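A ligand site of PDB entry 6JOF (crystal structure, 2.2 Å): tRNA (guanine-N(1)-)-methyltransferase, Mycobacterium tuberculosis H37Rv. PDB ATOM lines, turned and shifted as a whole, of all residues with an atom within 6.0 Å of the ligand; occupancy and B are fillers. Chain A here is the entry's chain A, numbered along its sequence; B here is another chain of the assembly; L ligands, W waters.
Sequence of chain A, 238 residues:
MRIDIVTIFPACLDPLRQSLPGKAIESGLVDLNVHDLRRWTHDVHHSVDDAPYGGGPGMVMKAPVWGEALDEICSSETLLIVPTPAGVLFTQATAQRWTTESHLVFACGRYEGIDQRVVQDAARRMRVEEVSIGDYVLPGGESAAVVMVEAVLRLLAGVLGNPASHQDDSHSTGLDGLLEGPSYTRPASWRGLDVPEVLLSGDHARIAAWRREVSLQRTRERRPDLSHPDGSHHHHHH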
ATOM      1  N   PRO A  57     -20.384   7.435 -23.961  1.00  0.00           N
ATOM      2  CA  PRO A  57     -21.249   7.911 -22.860  1.00  0.00           C
ATOM      3  C   PRO A  57     -21.005   7.147 -21.553  1.00  0.00           C
ATOM      4  O   PRO A  57     -20.329   6.113 -21.547  1.00  0.00           O
ATOM      5  CB  PRO A  57     -22.676   7.670 -23.390  1.00  0.00           C
ATOM      6  CG  PRO A  57     -22.518   7.278 -24.847  1.00  0.00           C
ATOM      7  CD  PRO A  57     -21.162   6.659 -24.943  1.00  0.00           C
ATOM      8  N   PRO A  83     -22.922 -10.277 -13.419  1.00  0.00           N
ATOM      9  CA  PRO A  83     -24.137 -10.021 -14.217  1.00  0.00           C
ATOM     10  C   PRO A  83     -23.852  -8.880 -15.208  1.00  0.00           C
ATOM     11  O   PRO A  83     -23.232  -7.880 -14.828  1.00  0.00           O
ATOM     12  CB  PRO A  83     -25.206  -9.666 -13.160  1.00  0.00           C
ATOM     13  CG  PRO A  83     -24.585  -9.972 -11.828  1.00  0.00           C
ATOM     14  CD  PRO A  83     -23.114  -9.848 -12.027  1.00  0.00           C
ATOM     15  N   THR A  84     -24.239  -9.062 -16.495  1.00  0.00           N
ATOM     16  CA  THR A  84     -23.966  -8.082 -17.565  1.00  0.00           C
ATOM     17  C   THR A  84     -24.890  -8.338 -18.769  1.00  0.00           C
ATOM     18  O   THR A  84     -25.175  -9.501 -19.021  1.00  0.00           O
ATOM     19  CB  THR A  84     -22.449  -8.121 -17.995  1.00  0.00           C
ATOM     20  OG1 THR A  84     -22.241  -7.339 -19.174  1.00  0.00           O
ATOM     21  CG2 THR A  84     -21.905  -9.526 -18.240  1.00  0.00           C
ATOM     22  N   PRO A  85     -25.309  -7.320 -19.574  1.00  0.00           N
ATOM     23  CA  PRO A  85     -26.128  -7.637 -20.766  1.00  0.00           C
ATOM     24  C   PRO A  85     -25.291  -8.273 -21.881  1.00  0.00           C
ATOM     25  O   PRO A  85     -25.821  -8.651 -22.905  1.00  0.00           O
ATOM     26  CB  PRO A  85     -26.701  -6.269 -21.180  1.00  0.00           C
ATOM     27  CG  PRO A  85     -25.669  -5.312 -20.746  1.00  0.00           C
ATOM     28  CD  PRO A  85     -25.053  -5.864 -19.486  1.00  0.00           C
ATOM     29  N   GLY A 109     -22.526  -4.858 -11.224  1.00  0.00           N
ATOM     30  CA  GLY A 109     -22.049  -3.652 -11.903  1.00  0.00           C
ATOM     31  C   GLY A 109     -23.086  -2.551 -12.039  1.00  0.00           C
ATOM     32  O   GLY A 109     -24.292  -2.811 -12.193  1.00  0.00           O
ATOM     33  N   ARG A 110     -22.601  -1.307 -11.971  1.00  0.00           N
ATOM     34  CA  ARG A 110     -23.385  -0.091 -12.181  1.00  0.00           C
ATOM     35  C   ARG A 110     -22.670   0.770 -13.225  1.00  0.00           C
ATOM     36  O   ARG A 110     -21.655   0.318 -13.775  1.00  0.00           O
ATOM     37  CB  ARG A 110     -23.665   0.652 -10.864  1.00  0.00           C
ATOM     38  CG  ARG A 110     -24.777   0.024 -10.029  1.00  0.00           C
ATOM     39  CD  ARG A 110     -26.168   0.541 -10.362  1.00  0.00           C
ATOM     40  NE  ARG A 110     -27.208  -0.311  -9.783  1.00  0.00           N
ATOM     41  CZ  ARG A 110     -28.505  -0.028  -9.801  1.00  0.00           C
ATOM     42  NH1 ARG A 110     -28.942   1.097 -10.359  1.00  0.00           N
ATOM     43  NH2 ARG A 110     -29.384  -0.858  -9.257  1.00  0.00           N
ATOM     44  N   TYR A 111     -23.218   1.969 -13.525  1.00  0.00           N
ATOM     45  CA  TYR A 111     -22.748   2.909 -14.565  1.00  0.00           C
ATOM     46  C   TYR A 111     -22.789   2.168 -15.923  1.00  0.00           C
ATOM     47  O   TYR A 111     -23.810   1.550 -16.207  1.00  0.00           O
ATOM     48  CB  TYR A 111     -21.386   3.540 -14.213  1.00  0.00           C
ATOM     49  CG  TYR A 111     -21.354   4.203 -12.852  1.00  0.00           C
ATOM     50  CD1 TYR A 111     -21.753   5.530 -12.695  1.00  0.00           C
ATOM     51  CD2 TYR A 111     -20.920   3.504 -11.721  1.00  0.00           C
ATOM     52  CE1 TYR A 111     -21.725   6.149 -11.435  1.00  0.00           C
ATOM     53  CE2 TYR A 111     -20.909   4.106 -10.466  1.00  0.00           C
ATOM     54  CZ  TYR A 111     -21.307   5.425 -10.326  1.00  0.00           C
ATOM     55  OH  TYR A 111     -21.287   6.040  -9.087  1.00  0.00           O
ATOM     56  N   GLU A 112     -21.691   2.160 -16.711  1.00  0.00           N
ATOM     57  CA  GLU A 112     -21.651   1.444 -17.999  1.00  0.00           C
ATOM     58  C   GLU A 112     -21.181   0.000 -17.875  1.00  0.00           C
ATOM     59  O   GLU A 112     -21.213  -0.756 -18.848  1.00  0.00           O
ATOM     60  CB  GLU A 112     -20.824   2.219 -19.052  1.00  0.00           C
ATOM     61  CG  GLU A 112     -21.571   3.395 -19.661  1.00  0.00           C
ATOM     62  CD  GLU A 112     -22.836   3.013 -20.404  1.00  0.00           C
ATOM     63  OE1 GLU A 112     -22.729   2.242 -21.384  1.00  0.00           O
ATOM     64  OE2 GLU A 112     -23.927   3.446 -19.982  1.00  0.00           O
ATOM     65  N   GLY A 113     -20.767  -0.375 -16.666  1.00  0.00           N
ATOM     66  CA  GLY A 113     -20.256  -1.698 -16.332  1.00  0.00           C
ATOM     67  C   GLY A 113     -18.906  -1.665 -15.652  1.00  0.00           C
ATOM     68  O   GLY A 113     -18.395  -0.601 -15.308  1.00  0.00           O
ATOM     69  N   VAL A 131     -22.983 -13.323 -17.120  1.00  0.00           N
ATOM     70  CA  VAL A 131     -24.329 -13.847 -17.323  1.00  0.00           C
ATOM     71  C   VAL A 131     -25.368 -12.733 -17.432  1.00  0.00           C
ATOM     72  O   VAL A 131     -25.342 -11.781 -16.652  1.00  0.00           O
ATOM     73  CB  VAL A 131     -24.647 -14.859 -16.163  1.00  0.00           C
ATOM     74  CG1 VAL A 131     -26.072 -15.412 -16.223  1.00  0.00           C
ATOM     75  CG2 VAL A 131     -23.631 -16.012 -16.114  1.00  0.00           C
ATOM     76  N   SER A 132     -26.278 -12.852 -18.423  1.00  0.00           N
ATOM     77  CA  SER A 132     -27.406 -11.949 -18.648  1.00  0.00           C
ATOM     78  C   SER A 132     -28.684 -12.673 -18.242  1.00  0.00           C
ATOM     79  O   SER A 132     -28.771 -13.875 -18.464  1.00  0.00           O
ATOM     80  CB  SER A 132     -27.493 -11.559 -20.123  1.00  0.00           C
ATOM     81  OG  SER A 132     -28.704 -10.873 -20.415  1.00  0.00           O
ATOM     82  N   ILE A 133     -29.679 -11.950 -17.687  1.00  0.00           N
ATOM     83  CA  ILE A 133     -30.964 -12.577 -17.317  1.00  0.00           C
ATOM     84  C   ILE A 133     -32.004 -12.476 -18.453  1.00  0.00           C
ATOM     85  O   ILE A 133     -33.043 -13.144 -18.382  1.00  0.00           O
ATOM     86  CB  ILE A 133     -31.550 -12.148 -15.946  1.00  0.00           C
ATOM     87  CG1 ILE A 133     -31.746 -10.613 -15.821  1.00  0.00           C
ATOM     88  CG2 ILE A 133     -30.705 -12.723 -14.796  1.00  0.00           C
ATOM     89  CD1 ILE A 133     -32.843 -10.178 -14.835  1.00  0.00           C
ATOM     90  N   GLY A 134     -31.696 -11.703 -19.512  1.00  0.00           N
ATOM     91  CA  GLY A 134     -32.584 -11.588 -20.657  1.00  0.00           C
ATOM     92  C   GLY A 134     -32.321 -10.464 -21.630  1.00  0.00           C
ATOM     93  O   GLY A 134     -31.471  -9.609 -21.390  1.00  0.00           O
ATOM     94  N   ASP A 135     -33.099 -10.437 -22.738  1.00  0.00           N
ATOM     95  CA  ASP A 135     -32.970  -9.460 -23.815  1.00  0.00           C
ATOM     96  C   ASP A 135     -33.631  -8.112 -23.505  1.00  0.00           C
ATOM     97  O   ASP A 135     -34.471  -7.642 -24.261  1.00  0.00           O
ATOM     98  CB  ASP A 135     -33.472 -10.056 -25.134  1.00  0.00           C
ATOM     99  CG  ASP A 135     -32.679 -11.259 -25.561  1.00  0.00           C
ATOM    100  OD1 ASP A 135     -31.483 -11.354 -25.184  1.00  0.00           O
ATOM    101  OD2 ASP A 135     -33.235 -12.129 -26.254  1.00  0.00           O
ATOM    102  N   TYR A 136     -33.186  -7.470 -22.421  1.00  0.00           N
ATOM    103  CA  TYR A 136     -33.692  -6.178 -21.976  1.00  0.00           C
ATOM    104  C   TYR A 136     -32.590  -5.466 -21.200  1.00  0.00           C
ATOM    105  O   TYR A 136     -31.678  -6.115 -20.709  1.00  0.00           O
ATOM    106  CB  TYR A 136     -34.989  -6.360 -21.141  1.00  0.00           C
ATOM    107  CG  TYR A 136     -34.931  -7.525 -20.187  1.00  0.00           C
ATOM    108  CD1 TYR A 136     -34.197  -7.445 -18.999  1.00  0.00           C
ATOM    109  CD2 TYR A 136     -35.545  -8.735 -20.489  1.00  0.00           C
ATOM    110  CE1 TYR A 136     -34.117  -8.524 -18.128  1.00  0.00           C
ATOM    111  CE2 TYR A 136     -35.469  -9.827 -19.624  1.00  0.00           C
ATOM    112  CZ  TYR A 136     -34.762  -9.712 -18.442  1.00  0.00           C
ATOM    113  OH  TYR A 136     -34.692 -10.792 -17.583  1.00  0.00           O
ATOM    114  N   VAL A 137     -32.678  -4.139 -21.092  1.00  0.00           N
ATOM    115  CA  VAL A 137     -31.657  -3.316 -20.428  1.00  0.00           C
ATOM    116  C   VAL A 137     -32.116  -2.821 -19.060  1.00  0.00           C
ATOM    117  O   VAL A 137     -33.172  -2.213 -18.941  1.00  0.00           O
ATOM    118  CB  VAL A 137     -31.204  -2.166 -21.370  1.00  0.00           C
ATOM    119  CG1 VAL A 137     -29.978  -1.451 -20.821  1.00  0.00           C
ATOM    120  CG2 VAL A 137     -30.936  -2.670 -22.789  1.00  0.00           C
ATOM    121  N   LEU A 138     -31.306  -3.117 -18.032  1.00  0.00           N
ATOM    122  CA  LEU A 138     -31.513  -2.750 -16.633  1.00  0.00           C
ATOM    123  C   LEU A 138     -30.486  -1.694 -16.201  1.00  0.00           C
ATOM    124  O   LEU A 138     -29.415  -1.630 -16.804  1.00  0.00           O
ATOM    125  CB  LEU A 138     -31.364  -4.010 -15.761  1.00  0.00           C
ATOM    126  CG  LEU A 138     -32.389  -5.116 -16.058  1.00  0.00           C
ATOM    127  CD1 LEU A 138     -31.843  -6.483 -15.756  1.00  0.00           C
ATOM    128  CD2 LEU A 138     -33.666  -4.871 -15.325  1.00  0.00           C
ATOM    129  N   PRO A 139     -30.782  -0.845 -15.180  1.00  0.00           N
ATOM    130  CA  PRO A 139     -29.797   0.171 -14.776  1.00  0.00           C
ATOM    131  C   PRO A 139     -28.634  -0.368 -13.913  1.00  0.00           C
ATOM    132  O   PRO A 139     -27.694   0.365 -13.655  1.00  0.00           O
ATOM    133  CB  PRO A 139     -30.651   1.167 -13.988  1.00  0.00           C
ATOM    134  CG  PRO A 139     -31.702   0.320 -13.356  1.00  0.00           C
ATOM    135  CD  PRO A 139     -32.001  -0.779 -14.348  1.00  0.00           C
ATOM    136  N   GLY A 140     -28.753  -1.617 -13.460  1.00  0.00           N
ATOM    137  CA  GLY A 140     -27.764  -2.262 -12.601  1.00  0.00           C
ATOM    138  C   GLY A 140     -27.892  -3.771 -12.580  1.00  0.00           C
ATOM    139  O   GLY A 140     -28.786  -4.327 -13.230  1.00  0.00           O
ATOM    140  N   GLY A 141     -26.975  -4.430 -11.862  1.00  0.00           N
ATOM    141  CA  GLY A 141     -26.913  -5.901 -11.782  1.00  0.00           C
ATOM    142  C   GLY A 141     -27.489  -6.533 -10.527  1.00  0.00           C
ATOM    143  O   GLY A 141     -27.432  -7.758 -10.387  1.00  0.00           O
ATOM    144  N   GLU A 142     -28.045  -5.710  -9.619  1.00  0.00           N
ATOM    145  CA  GLU A 142     -28.603  -6.153  -8.353  1.00  0.00           C
ATOM    146  C   GLU A 142     -29.905  -6.891  -8.497  1.00  0.00           C
ATOM    147  O   GLU A 142     -30.071  -7.912  -7.833  1.00  0.00           O
ATOM    148  CB  GLU A 142     -28.737  -5.015  -7.338  1.00  0.00           C
ATOM    149  CG  GLU A 142     -27.417  -4.377  -6.936  1.00  0.00           C
ATOM    150  CD  GLU A 142     -26.849  -3.312  -7.853  1.00  0.00           C
ATOM    151  OE1 GLU A 142     -27.491  -2.979  -8.877  1.00  0.00           O
ATOM    152  OE2 GLU A 142     -25.768  -2.772  -7.539  1.00  0.00           O
ATOM    153  N   ALA A 144     -30.871  -8.472 -11.203  1.00  0.00           N
ATOM    154  CA  ALA A 144     -30.436  -9.699 -11.882  1.00  0.00           C
ATOM    155  C   ALA A 144     -29.894 -10.699 -10.868  1.00  0.00           C
ATOM    156  O   ALA A 144     -30.202 -11.879 -10.968  1.00  0.00           O
ATOM    157  CB  ALA A 144     -29.392  -9.373 -12.932  1.00  0.00           C
ATOM    158  N   MET A 148     -31.230 -14.585  -9.975  1.00  0.00           N
ATOM    159  CA  MET A 148     -30.319 -15.724 -10.016  1.00  0.00           C
ATOM    160  C   MET A 148     -30.192 -16.438  -8.650  1.00  0.00           C
ATOM    161  O   MET A 148     -30.126 -17.673  -8.604  1.00  0.00           O
ATOM    162  CB  MET A 148     -28.925 -15.318 -10.563  1.00  0.00           C
ATOM    163  CG  MET A 148     -28.937 -14.809 -12.013  1.00  0.00           C
ATOM    164  SD  MET A 148     -27.284 -14.457 -12.709  1.00  0.00           S
ATOM    165  CE  MET A 148     -27.024 -12.842 -12.153  1.00  0.00           C
ATOM    166  N   ARG B 154     -36.029   3.059 -16.402  1.00  0.00           N
ATOM    167  CA  ARG B 154     -34.723   3.437 -16.952  1.00  0.00           C
ATOM    168  C   ARG B 154     -34.934   4.327 -18.183  1.00  0.00           C
ATOM    169  O   ARG B 154     -34.248   5.338 -18.326  1.00  0.00           O
ATOM    170  CB  ARG B 154     -33.933   2.166 -17.347  1.00  0.00           C
ATOM    171  CG  ARG B 154     -32.473   2.433 -17.670  1.00  0.00           C
ATOM    172  CD  ARG B 154     -31.760   1.204 -18.222  1.00  0.00           C
ATOM    173  NE  ARG B 154     -30.754   1.596 -19.195  1.00  0.00           N
ATOM    174  CZ  ARG B 154     -30.998   1.759 -20.493  1.00  0.00           C
ATOM    175  NH1 ARG B 154     -32.206   1.508 -20.984  1.00  0.00           N
ATOM    176  NH2 ARG B 154     -30.028   2.153 -21.313  1.00  0.00           N
ATOM    177  N   GLU B 180     -23.043  -5.782 -26.018  1.00  0.00           N
ATOM    178  CA  GLU B 180     -22.176  -4.650 -25.709  1.00  0.00           C
ATOM    179  C   GLU B 180     -20.748  -5.146 -25.583  1.00  0.00           C
ATOM    180  O   GLU B 180     -20.512  -6.201 -24.992  1.00  0.00           O
ATOM    181  CB  GLU B 180     -22.605  -3.955 -24.400  1.00  0.00           C
ATOM    182  CG  GLU B 180     -23.402  -2.678 -24.596  1.00  0.00           C
ATOM    183  CD  GLU B 180     -24.876  -2.858 -24.880  1.00  0.00           C
ATOM    184  OE1 GLU B 180     -25.610  -3.292 -23.961  1.00  0.00           O
ATOM    185  OE2 GLU B 180     -25.313  -2.514 -25.998  1.00  0.00           O
HETATM  186  C1  LIG L   1     -26.965   0.117 -23.381  1.00  0.00           C
HETATM  187  C2  LIG L   1     -27.895   1.234 -23.929  1.00  0.00           C
HETATM  188  C3  LIG L   1     -27.066   2.365 -24.586  1.00  0.00           C
HETATM  189  N1  LIG L   1     -27.930   3.492 -24.980  1.00  0.00           N
HETATM  190  C4  LIG L   1     -25.905   2.845 -23.663  1.00  0.00           C
HETATM  191  C5  LIG L   1     -25.109   1.633 -23.133  1.00  0.00           C
HETATM  192  N2  LIG L   1     -25.951   0.641 -22.421  1.00  0.00           N
HETATM  193  C6  LIG L   1     -25.047  -0.441 -21.936  1.00  0.00           C
HETATM  194  C7  LIG L   1     -25.363  -0.997 -20.670  1.00  0.00           C
HETATM  195  C8  LIG L   1     -24.407  -1.022 -19.652  1.00  0.00           C
HETATM  196  C9  LIG L   1     -24.706  -1.610 -18.415  1.00  0.00           C
HETATM  197  C10 LIG L   1     -26.598  -1.612 -20.435  1.00  0.00           C
HETATM  198  C11 LIG L   1     -26.907  -2.193 -19.191  1.00  0.00           C
HETATM  199  C12 LIG L   1     -25.948  -2.205 -18.168  1.00  0.00           C
HETATM  200  C13 LIG L   1     -26.235  -2.780 -16.914  1.00  0.00           C
HETATM  201  N3  LIG L   1     -26.730  -4.182 -17.019  1.00  0.00           N
HETATM  202  C14 LIG L   1     -26.726  -5.089 -16.012  1.00  0.00           C
HETATM  203  O1  LIG L   1     -26.145  -4.868 -14.955  1.00  0.00           O
HETATM  204  C15 LIG L   1     -27.205  -6.358 -16.235  1.00  0.00           C
HETATM  205  C16 LIG L   1     -28.171  -6.824 -17.120  1.00  0.00           C
HETATM  206  C17 LIG L   1     -28.904  -6.246 -18.133  1.00  0.00           C
HETATM  207  O2  LIG L   1     -28.876  -5.045 -18.391  1.00  0.00           O
HETATM  208  N4  LIG L   1     -29.793  -6.998 -18.945  1.00  0.00           N
HETATM  209  C18 LIG L   1     -29.953  -8.296 -18.759  1.00  0.00           C
HETATM  210  N5  LIG L   1     -29.210  -8.903 -17.743  1.00  0.00           N
HETATM  211  C19 LIG L   1     -28.377  -8.170 -16.959  1.00  0.00           C
HETATM  212  S1  LIG L   1     -27.440  -8.751 -15.745  1.00  0.00           S
HETATM  213  C20 LIG L   1     -26.759  -7.287 -15.393  1.00  0.00           C
HETATM  214  O   HOH W   1     -24.061  -6.023 -13.272  1.00  0.00           O
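OG of Ser 132 sits close to N5 of the ligand, at 3.4 Å. N of Thr 84 sits close to S1 of the ligand (3.3 Å). An oxygen (O1) of the ligand lies within hydrogen-bond range of the backbone NH (N) of Gly 141 (3.2 Å). N of Leu 138 sits at hydrogen-bond distance from O2 of the ligand, at 3.1 Å. A nitrogen (N2) of the ligand lies within salt-bridge range of the side-chain carboxylate (OE1) of Glu 112 (3.7 Å). N of Ile 133 is in hydrogen-bond range of N5 of the ligand. The backbone carbonyl oxygen of Tyr 136 sits at hydrogen-bond distance from a nitrogen (N4) of the ligand (2.7 Å).
OH of Tyr 136 lies within hydrogen-bond range of O of Ile 133, at 3.0 Å. OG of Ser 132 is in hydrogen-bond range of O of Gly 134, 3.2 Å away. The backbone NH of Thr 84 is in hydrogen-bond range of the backbone carbonyl oxygen of Val 131, at 2.9 Å. The backbone NH (N) of Gly 141 is in hydrogen-bond range of the backbone carbonyl oxygen (O) of Gly 109.
Water W1 lies within hydrogen-bond range of the backbone carbonyl oxygen of Pro 83 (2.6 Å), the backbone NH of Gly 109 (2.8 Å) and an oxygen (O1) of the ligand (2.9 Å).
O of Val 131 lies close to S1 of the ligand, 3.8 Å away. The backbone carbonyl oxygen of Gly 140 lies close to an oxygen (O1) of the ligand (3.2 Å). Pro 83 touches the ligand. Pro 85 touches the ligand. O of Gly 109 touches O1 of the ligand (3.9 Å). Tyr 111 touches the ligand. Gly 134 touches the ligand. Val 137 touches the ligand. CB of Ala 144 touches S1 of the ligand, 3.5 Å away. Arg 154 of chain B touches the ligand (NH2 to C2, 3.5 Å). OE1 of Glu 180 of chain B touches C6 of the ligand, at 3.5 Å. Hydrophobic or aromatic side chains within 4 Å of the ligand: Pro 83, Pro 85, Ile 133, Val 137, Leu 138 and Ala 144. Along chain A the residues within 4 Å of the ligand span positions 83 to 144. The nearest printed residue that does not touch the ligand is Gly 113 (4.5 Å).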
